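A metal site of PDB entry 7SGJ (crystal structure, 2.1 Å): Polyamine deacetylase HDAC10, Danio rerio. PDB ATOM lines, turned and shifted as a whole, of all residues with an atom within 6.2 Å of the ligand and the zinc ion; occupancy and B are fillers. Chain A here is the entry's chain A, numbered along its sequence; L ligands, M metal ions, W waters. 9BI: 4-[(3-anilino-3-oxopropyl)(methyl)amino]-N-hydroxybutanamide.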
ATOM      1  N   GLU A  24     -30.177  -6.165 -26.134  1.00  0.00           N
ATOM      2  CA  GLU A  24     -29.717  -4.907 -26.696  1.00  0.00           C
ATOM      3  C   GLU A  24     -28.472  -4.361 -25.993  1.00  0.00           C
ATOM      4  O   GLU A  24     -27.914  -3.376 -26.465  1.00  0.00           O
ATOM      5  CB  GLU A  24     -30.849  -3.860 -26.640  1.00  0.00           C
ATOM      6  CG  GLU A  24     -32.097  -4.206 -27.466  1.00  0.00           C
ATOM      7  CD  GLU A  24     -31.785  -4.881 -28.816  1.00  0.00           C
ATOM      8  OE1 GLU A  24     -32.410  -5.932 -29.102  1.00  0.00           O
ATOM      9  OE2 GLU A  24     -30.934  -4.374 -29.588  1.00  0.00           O
ATOM     10  N   CYS A  25     -28.024  -4.986 -24.901  1.00  0.00           N
ATOM     11  CA  CYS A  25     -26.864  -4.518 -24.168  1.00  0.00           C
ATOM     12  C   CYS A  25     -25.753  -5.558 -24.020  1.00  0.00           C
ATOM     13  O   CYS A  25     -24.644  -5.179 -23.609  1.00  0.00           O
ATOM     14  CB  CYS A  25     -27.277  -4.025 -22.757  1.00  0.00           C
ATOM     15  SG  CYS A  25     -28.289  -2.485 -22.750  1.00  0.00           S
ATOM     16  N   ILE A  27     -23.581  -6.882 -25.824  1.00  0.00           N
ATOM     17  CA  ILE A  27     -22.305  -6.719 -26.518  1.00  0.00           C
ATOM     18  C   ILE A  27     -21.339  -5.814 -25.781  1.00  0.00           C
ATOM     19  O   ILE A  27     -20.147  -5.771 -26.140  1.00  0.00           O
ATOM     20  CB  ILE A  27     -22.540  -6.151 -27.927  1.00  0.00           C
ATOM     21  CG1 ILE A  27     -23.396  -4.877 -27.823  1.00  0.00           C
ATOM     22  CG2 ILE A  27     -23.191  -7.197 -28.836  1.00  0.00           C
ATOM     23  CD1 ILE A  27     -23.370  -4.005 -29.048  1.00  0.00           C
ATOM     24  N   ASN A  93     -32.695   4.645 -22.445  1.00  0.00           N
ATOM     25  CA  ASN A  93     -32.684   3.823 -23.644  1.00  0.00           C
ATOM     26  C   ASN A  93     -31.311   3.153 -23.816  1.00  0.00           C
ATOM     27  O   ASN A  93     -30.289   3.851 -23.884  1.00  0.00           O
ATOM     28  CB  ASN A  93     -33.000   4.657 -24.884  1.00  0.00           C
ATOM     29  CG  ASN A  93     -33.144   3.817 -26.124  1.00  0.00           C
ATOM     30  OD1 ASN A  93     -32.317   3.871 -27.033  1.00  0.00           O
ATOM     31  ND2 ASN A  93     -34.196   2.996 -26.170  1.00  0.00           N
ATOM     32  N   ALA A  94     -31.309   1.822 -23.927  1.00  0.00           N
ATOM     33  CA  ALA A  94     -30.134   1.016 -24.284  1.00  0.00           C
ATOM     34  C   ALA A  94     -28.939   1.277 -23.353  1.00  0.00           C
ATOM     35  O   ALA A  94     -27.835   1.611 -23.792  1.00  0.00           O
ATOM     36  CB  ALA A  94     -29.763   1.241 -25.750  1.00  0.00           C
ATOM     37  N   PRO A 134     -18.412   4.073 -22.442  1.00  0.00           N
ATOM     38  CA  PRO A 134     -18.300   5.114 -23.474  1.00  0.00           C
ATOM     39  C   PRO A 134     -19.146   6.340 -23.114  1.00  0.00           C
ATOM     40  O   PRO A 134     -19.897   6.355 -22.129  1.00  0.00           O
ATOM     41  CB  PRO A 134     -18.807   4.438 -24.746  1.00  0.00           C
ATOM     42  CG  PRO A 134     -19.803   3.393 -24.222  1.00  0.00           C
ATOM     43  CD  PRO A 134     -19.146   2.887 -22.938  1.00  0.00           C
ATOM     44  N   HIS A 136     -20.425   9.041 -25.913  1.00  0.00           N
ATOM     45  CA  HIS A 136     -20.895  10.033 -26.889  1.00  0.00           C
ATOM     46  C   HIS A 136     -22.420  10.079 -27.004  1.00  0.00           C
ATOM     47  O   HIS A 136     -22.942  11.096 -27.487  1.00  0.00           O
ATOM     48  CB  HIS A 136     -20.228   9.821 -28.282  1.00  0.00           C
ATOM     49  CG  HIS A 136     -20.620   8.571 -29.009  1.00  0.00           C
ATOM     50  ND1 HIS A 136     -20.613   8.494 -30.393  1.00  0.00           N
ATOM     51  CD2 HIS A 136     -20.962   7.329 -28.567  1.00  0.00           C
ATOM     52  CE1 HIS A 136     -20.966   7.275 -30.771  1.00  0.00           C
ATOM     53  NE2 HIS A 136     -21.175   6.543 -29.678  1.00  0.00           N
ATOM     54  N   HIS A 137     -23.155   9.090 -26.496  1.00  0.00           N
ATOM     55  CA  HIS A 137     -24.610   9.179 -26.444  1.00  0.00           C
ATOM     56  C   HIS A 137     -25.139   9.865 -25.205  1.00  0.00           C
ATOM     57  O   HIS A 137     -26.333  10.195 -25.157  1.00  0.00           O
ATOM     58  CB  HIS A 137     -25.227   7.787 -26.532  1.00  0.00           C
ATOM     59  CG  HIS A 137     -24.895   7.071 -27.803  1.00  0.00           C
ATOM     60  ND1 HIS A 137     -25.082   7.657 -29.041  1.00  0.00           N
ATOM     61  CD2 HIS A 137     -24.354   5.859 -28.029  1.00  0.00           C
ATOM     62  CE1 HIS A 137     -24.658   6.817 -29.976  1.00  0.00           C
ATOM     63  NE2 HIS A 137     -24.219   5.720 -29.385  1.00  0.00           N
ATOM     64  N   GLY A 145     -27.448   4.556 -24.605  1.00  0.00           N
ATOM     65  CA  GLY A 145     -26.534   3.818 -25.484  1.00  0.00           C
ATOM     66  C   GLY A 145     -25.216   3.419 -24.828  1.00  0.00           C
ATOM     67  O   GLY A 145     -24.151   3.737 -25.358  1.00  0.00           O
ATOM     68  N   PHE A 146     -25.294   2.750 -23.675  1.00  0.00           N
ATOM     69  CA  PHE A 146     -24.166   2.275 -22.873  1.00  0.00           C
ATOM     70  C   PHE A 146     -23.368   3.411 -22.229  1.00  0.00           C
ATOM     71  O   PHE A 146     -22.401   3.121 -21.506  1.00  0.00           O
ATOM     72  CB  PHE A 146     -23.167   1.404 -23.668  1.00  0.00           C
ATOM     73  CG  PHE A 146     -23.819   0.375 -24.576  1.00  0.00           C
ATOM     74  CD1 PHE A 146     -25.035  -0.211 -24.237  1.00  0.00           C
ATOM     75  CD2 PHE A 146     -23.193  -0.011 -25.751  1.00  0.00           C
ATOM     76  CE1 PHE A 146     -25.619  -1.143 -25.070  1.00  0.00           C
ATOM     77  CE2 PHE A 146     -23.770  -0.955 -26.570  1.00  0.00           C
ATOM     78  CZ  PHE A 146     -24.992  -1.518 -26.223  1.00  0.00           C
ATOM     79  N   CYS A 147     -23.722   4.678 -22.463  1.00  0.00           N
ATOM     80  CA  CYS A 147     -22.996   5.841 -21.969  1.00  0.00           C
ATOM     81  C   CYS A 147     -23.683   6.439 -20.745  1.00  0.00           C
ATOM     82  O   CYS A 147     -24.898   6.636 -20.753  1.00  0.00           O
ATOM     83  CB  CYS A 147     -22.879   6.918 -23.041  1.00  0.00           C
ATOM     84  SG  CYS A 147     -22.236   6.323 -24.584  1.00  0.00           S
ATOM     85  N   ASP A 174     -16.990   6.578 -34.517  1.00  0.00           N
ATOM     86  CA  ASP A 174     -17.858   5.480 -34.092  1.00  0.00           C
ATOM     87  C   ASP A 174     -18.958   5.299 -35.138  1.00  0.00           C
ATOM     88  O   ASP A 174     -19.274   6.239 -35.883  1.00  0.00           O
ATOM     89  CB  ASP A 174     -18.468   5.803 -32.704  1.00  0.00           C
ATOM     90  CG  ASP A 174     -19.242   4.644 -32.099  1.00  0.00           C
ATOM     91  OD1 ASP A 174     -18.718   3.967 -31.192  1.00  0.00           O
ATOM     92  OD2 ASP A 174     -20.416   4.413 -32.471  1.00  0.00           O
ATOM     93  N   VAL A 175     -19.525   4.092 -35.208  1.00  0.00           N
ATOM     94  CA  VAL A 175     -20.522   3.836 -36.250  1.00  0.00           C
ATOM     95  C   VAL A 175     -21.901   4.356 -35.883  1.00  0.00           C
ATOM     96  O   VAL A 175     -22.805   4.362 -36.728  1.00  0.00           O
ATOM     97  CB  VAL A 175     -20.594   2.325 -36.581  1.00  0.00           C
ATOM     98  CG1 VAL A 175     -21.550   1.587 -35.637  1.00  0.00           C
ATOM     99  CG2 VAL A 175     -21.004   2.135 -38.048  1.00  0.00           C
ATOM    100  N   HIS A 176     -22.099   4.792 -34.640  1.00  0.00           N
ATOM    101  CA  HIS A 176     -23.362   5.340 -34.180  1.00  0.00           C
ATOM    102  C   HIS A 176     -23.245   6.852 -34.085  1.00  0.00           C
ATOM    103  O   HIS A 176     -22.160   7.410 -33.886  1.00  0.00           O
ATOM    104  CB  HIS A 176     -23.754   4.771 -32.820  1.00  0.00           C
ATOM    105  CG  HIS A 176     -23.988   3.295 -32.806  1.00  0.00           C
ATOM    106  ND1 HIS A 176     -22.997   2.387 -32.498  1.00  0.00           N
ATOM    107  CD2 HIS A 176     -25.104   2.564 -33.036  1.00  0.00           C
ATOM    108  CE1 HIS A 176     -23.495   1.162 -32.531  1.00  0.00           C
ATOM    109  NE2 HIS A 176     -24.767   1.247 -32.863  1.00  0.00           N
ATOM    110  N   TRP A 205     -30.853   2.659 -35.028  1.00  0.00           N
ATOM    111  CA  TRP A 205     -30.712   3.283 -33.717  1.00  0.00           C
ATOM    112  C   TRP A 205     -29.628   4.367 -33.758  1.00  0.00           C
ATOM    113  O   TRP A 205     -28.573   4.167 -34.362  1.00  0.00           O
ATOM    114  CB  TRP A 205     -30.373   2.201 -32.674  1.00  0.00           C
ATOM    115  CG  TRP A 205     -30.452   2.698 -31.272  1.00  0.00           C
ATOM    116  CD1 TRP A 205     -31.546   2.631 -30.432  1.00  0.00           C
ATOM    117  CD2 TRP A 205     -29.436   3.402 -30.556  1.00  0.00           C
ATOM    118  NE1 TRP A 205     -31.246   3.248 -29.236  1.00  0.00           N
ATOM    119  CE2 TRP A 205     -29.969   3.746 -29.293  1.00  0.00           C
ATOM    120  CE3 TRP A 205     -28.129   3.792 -30.876  1.00  0.00           C
ATOM    121  CZ2 TRP A 205     -29.231   4.440 -28.327  1.00  0.00           C
ATOM    122  CZ3 TRP A 205     -27.378   4.486 -29.916  1.00  0.00           C
ATOM    123  CH2 TRP A 205     -27.940   4.801 -28.649  1.00  0.00           C
ATOM    124  N   ASN A 207     -32.273   6.339 -34.281  1.00  0.00           N
ATOM    125  CA  ASN A 207     -33.497   6.661 -35.027  1.00  0.00           C
ATOM    126  C   ASN A 207     -33.879   8.137 -34.916  1.00  0.00           C
ATOM    127  O   ASN A 207     -35.034   8.455 -34.650  1.00  0.00           O
ATOM    128  CB  ASN A 207     -34.681   5.783 -34.557  1.00  0.00           C
ATOM    129  CG  ASN A 207     -34.335   4.318 -34.480  1.00  0.00           C
ATOM    130  OD1 ASN A 207     -34.084   3.777 -33.396  1.00  0.00           O
ATOM    131  ND2 ASN A 207     -34.352   3.646 -35.628  1.00  0.00           N
ATOM    132  N   GLY A 265     -14.870   5.112 -31.870  1.00  0.00           N
ATOM    133  CA  GLY A 265     -15.556   3.836 -31.806  1.00  0.00           C
ATOM    134  C   GLY A 265     -15.160   3.020 -33.022  1.00  0.00           C
ATOM    135  O   GLY A 265     -15.145   3.531 -34.153  1.00  0.00           O
ATOM    136  N   ASP A 267     -16.653   0.163 -33.796  1.00  0.00           N
ATOM    137  CA  ASP A 267     -17.755  -0.570 -34.373  1.00  0.00           C
ATOM    138  C   ASP A 267     -18.018  -0.146 -35.818  1.00  0.00           C
ATOM    139  O   ASP A 267     -18.928  -0.689 -36.438  1.00  0.00           O
ATOM    140  CB  ASP A 267     -19.029  -0.425 -33.527  1.00  0.00           C
ATOM    141  CG  ASP A 267     -19.343   1.003 -33.131  1.00  0.00           C
ATOM    142  OD1 ASP A 267     -18.777   1.962 -33.696  1.00  0.00           O
ATOM    143  OD2 ASP A 267     -20.206   1.140 -32.243  1.00  0.00           O
ATOM    144  N   GLU A 274     -22.650  -4.522 -34.791  1.00  0.00           N
ATOM    145  CA  GLU A 274     -23.490  -3.338 -34.781  1.00  0.00           C
ATOM    146  C   GLU A 274     -23.403  -2.549 -36.087  1.00  0.00           C
ATOM    147  O   GLU A 274     -24.422  -2.120 -36.633  1.00  0.00           O
ATOM    148  CB  GLU A 274     -23.130  -2.425 -33.605  1.00  0.00           C
ATOM    149  CG  GLU A 274     -23.809  -2.804 -32.331  1.00  0.00           C
ATOM    150  CD  GLU A 274     -25.309  -2.580 -32.394  1.00  0.00           C
ATOM    151  OE1 GLU A 274     -25.734  -1.428 -32.676  1.00  0.00           O
ATOM    152  OE2 GLU A 274     -26.052  -3.555 -32.158  1.00  0.00           O
ATOM    153  N   GLU A 304     -14.730   4.871 -27.733  1.00  0.00           N
ATOM    154  CA  GLU A 304     -16.188   4.778 -27.608  1.00  0.00           C
ATOM    155  C   GLU A 304     -16.613   3.314 -27.718  1.00  0.00           C
ATOM    156  O   GLU A 304     -16.386   2.529 -26.794  1.00  0.00           O
ATOM    157  CB  GLU A 304     -16.883   5.647 -28.651  1.00  0.00           C
ATOM    158  CG  GLU A 304     -16.542   7.139 -28.537  1.00  0.00           C
ATOM    159  CD  GLU A 304     -17.304   7.860 -27.411  1.00  0.00           C
ATOM    160  OE1 GLU A 304     -18.158   7.241 -26.743  1.00  0.00           O
ATOM    161  OE2 GLU A 304     -17.053   9.082 -27.216  1.00  0.00           O
ATOM    162  N   GLY A 305     -17.211   2.922 -28.843  1.00  0.00           N
ATOM    163  CA  GLY A 305     -17.693   1.559 -29.064  1.00  0.00           C
ATOM    164  C   GLY A 305     -16.710   0.686 -29.825  1.00  0.00           C
ATOM    165  O   GLY A 305     -15.540   1.037 -30.034  1.00  0.00           O
ATOM    166  N   GLY A 306     -17.205  -0.481 -30.262  1.00  0.00           N
ATOM    167  CA  GLY A 306     -16.407  -1.484 -30.978  1.00  0.00           C
ATOM    168  C   GLY A 306     -16.510  -2.845 -30.304  1.00  0.00           C
ATOM    169  O   GLY A 306     -15.988  -3.007 -29.211  1.00  0.00           O
ATOM    170  N   TYR A 307     -17.157  -3.829 -30.947  1.00  0.00           N
ATOM    171  CA  TYR A 307     -17.678  -4.999 -30.233  1.00  0.00           C
ATOM    172  C   TYR A 307     -17.213  -6.353 -30.758  1.00  0.00           C
ATOM    173  O   TYR A 307     -17.443  -7.352 -30.074  1.00  0.00           O
ATOM    174  CB  TYR A 307     -19.210  -4.968 -30.220  1.00  0.00           C
ATOM    175  CG  TYR A 307     -19.693  -3.644 -29.670  1.00  0.00           C
ATOM    176  CD1 TYR A 307     -19.637  -3.393 -28.309  1.00  0.00           C
ATOM    177  CD2 TYR A 307     -20.122  -2.633 -30.512  1.00  0.00           C
ATOM    178  CE1 TYR A 307     -20.025  -2.176 -27.793  1.00  0.00           C
ATOM    179  CE2 TYR A 307     -20.533  -1.416 -30.014  1.00  0.00           C
ATOM    180  CZ  TYR A 307     -20.476  -1.199 -28.653  1.00  0.00           C
ATOM    181  OH  TYR A 307     -20.857   0.012 -28.158  1.00  0.00           O
HETATM  182  C10 9BI L   1     -28.819  -0.142 -28.932  1.00  0.00           C
HETATM  183  C15 9BI L   1     -33.750  -0.920 -29.681  1.00  0.00           C
HETATM  184  C17 9BI L   1     -35.964  -1.846 -29.431  1.00  0.00           C
HETATM  185  C20 9BI L   1     -34.156   0.216 -28.977  1.00  0.00           C
HETATM  186  C01 9BI L   1     -26.957  -1.511 -29.478  1.00  0.00           C
HETATM  187  C03 9BI L   1     -26.624   0.761 -28.757  1.00  0.00           C
HETATM  188  C04 9BI L   1     -25.261   0.971 -29.425  1.00  0.00           C
HETATM  189  C05 9BI L   1     -24.427   2.042 -28.699  1.00  0.00           C
HETATM  190  C06 9BI L   1     -23.027   2.284 -29.262  1.00  0.00           C
HETATM  191  C11 9BI L   1     -29.801  -1.010 -29.741  1.00  0.00           C
HETATM  192  C12 9BI L   1     -31.253  -0.911 -29.246  1.00  0.00           C
HETATM  193  C16 9BI L   1     -34.660  -1.954 -29.894  1.00  0.00           C
HETATM  194  C18 9BI L   1     -36.370  -0.710 -28.727  1.00  0.00           C
HETATM  195  C19 9BI L   1     -35.470   0.318 -28.501  1.00  0.00           C
HETATM  196  N02 9BI L   1     -27.481  -0.154 -29.510  1.00  0.00           N
HETATM  197  N08 9BI L   1     -22.596   3.647 -29.468  1.00  0.00           N
HETATM  198  N14 9BI L   1     -32.380  -1.027 -30.172  1.00  0.00           N
HETATM  199  O07 9BI L   1     -22.293   1.401 -29.540  1.00  0.00           O
HETATM  200  O09 9BI L   1     -21.338   4.001 -29.959  1.00  0.00           O
HETATM  201  O13 9BI L   1     -31.468  -0.744 -28.078  1.00  0.00           O
HETATM  202 ZN    ZN M   1     -21.069   2.826 -31.586  1.00  0.00          ZN
HETATM  203  O   HOH W   1     -27.972  -0.088 -32.312  1.00  0.00           O
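N of Gly 145 lies within hydrogen-bond range of O of Asn 93 (3.0 Å). A ring nitrogen (NE2) of His 137 is in hydrogen-bond range of a ring nitrogen (NE2) of His 136, 3.2 Å away. The backbone carbonyl oxygen (O) of Gly 145 sits at hydrogen-bond distance from the side-chain sulfur (SG) of Cys 147 (3.3 Å). The backbone carbonyl oxygen of Ala 94 is in hydrogen-bond range of the backbone NH of Phe 146 (2.8 Å). OD1 of Asn 93 lies within hydrogen-bond range of NE1 of Trp 205, at 2.5 Å. OD1 of Asp 174 sits at hydrogen-bond distance from N of Gly 305, 3.0 Å away. SG of Cys 147 sits at hydrogen-bond distance from N of His 137, at 3.5 Å. A ring nitrogen (NE2) of His 176 lies within hydrogen-bond range of the side-chain carboxylate (OE1) of Glu 274 (2.9 Å).
Three residues have an atom within 4 Å of the zinc ion: Asp 174, His 176 and Asp 267. Along chain A the residues within 4 Å of the zinc ion span positions 174 to 267.
NE2 of His 137 sits at hydrogen-bond distance from N08 of the ligand, 2.6 Å away. The side-chain carboxylate of Glu 274 lies within salt-bridge range of a nitrogen (N02) of the ligand (3.8 Å). N08 of the ligand sits at hydrogen-bond distance from NE2 of His 136 (3.2 Å). OH of Tyr 307 is in hydrogen-bond range of O07 of the ligand (2.4 Å).
The side-chain carboxylate (OD2) of Asp 174 binds the zinc ion (1.9 Å). The zinc ion is bound by OD2 of Asp 267. The zinc ion is bound by O09 of the ligand (2.0 Å). A ring nitrogen (ND1) of His 176 is bound to the zinc ion. Slightly farther from the zinc ion lies the side-chain carboxylate (OD1) of Asp 174 (2.6 Å). Slightly farther from the zinc ion lies O07 of the ligand (2.8 Å).
Merely in contact with the ligand: Glu 24 (3.5 Å), Ala 94 (3.5 Å), Phe 146 (3.7 Å), Trp 205 (3.7 Å), Gly 145 (3.8 Å) and Asn 93 (3.8 Å). Hydrophobic or aromatic side chains that line the ligand: Ala 94, His 136, His 137, Phe 146, His 176, Trp 205 and Tyr 307.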
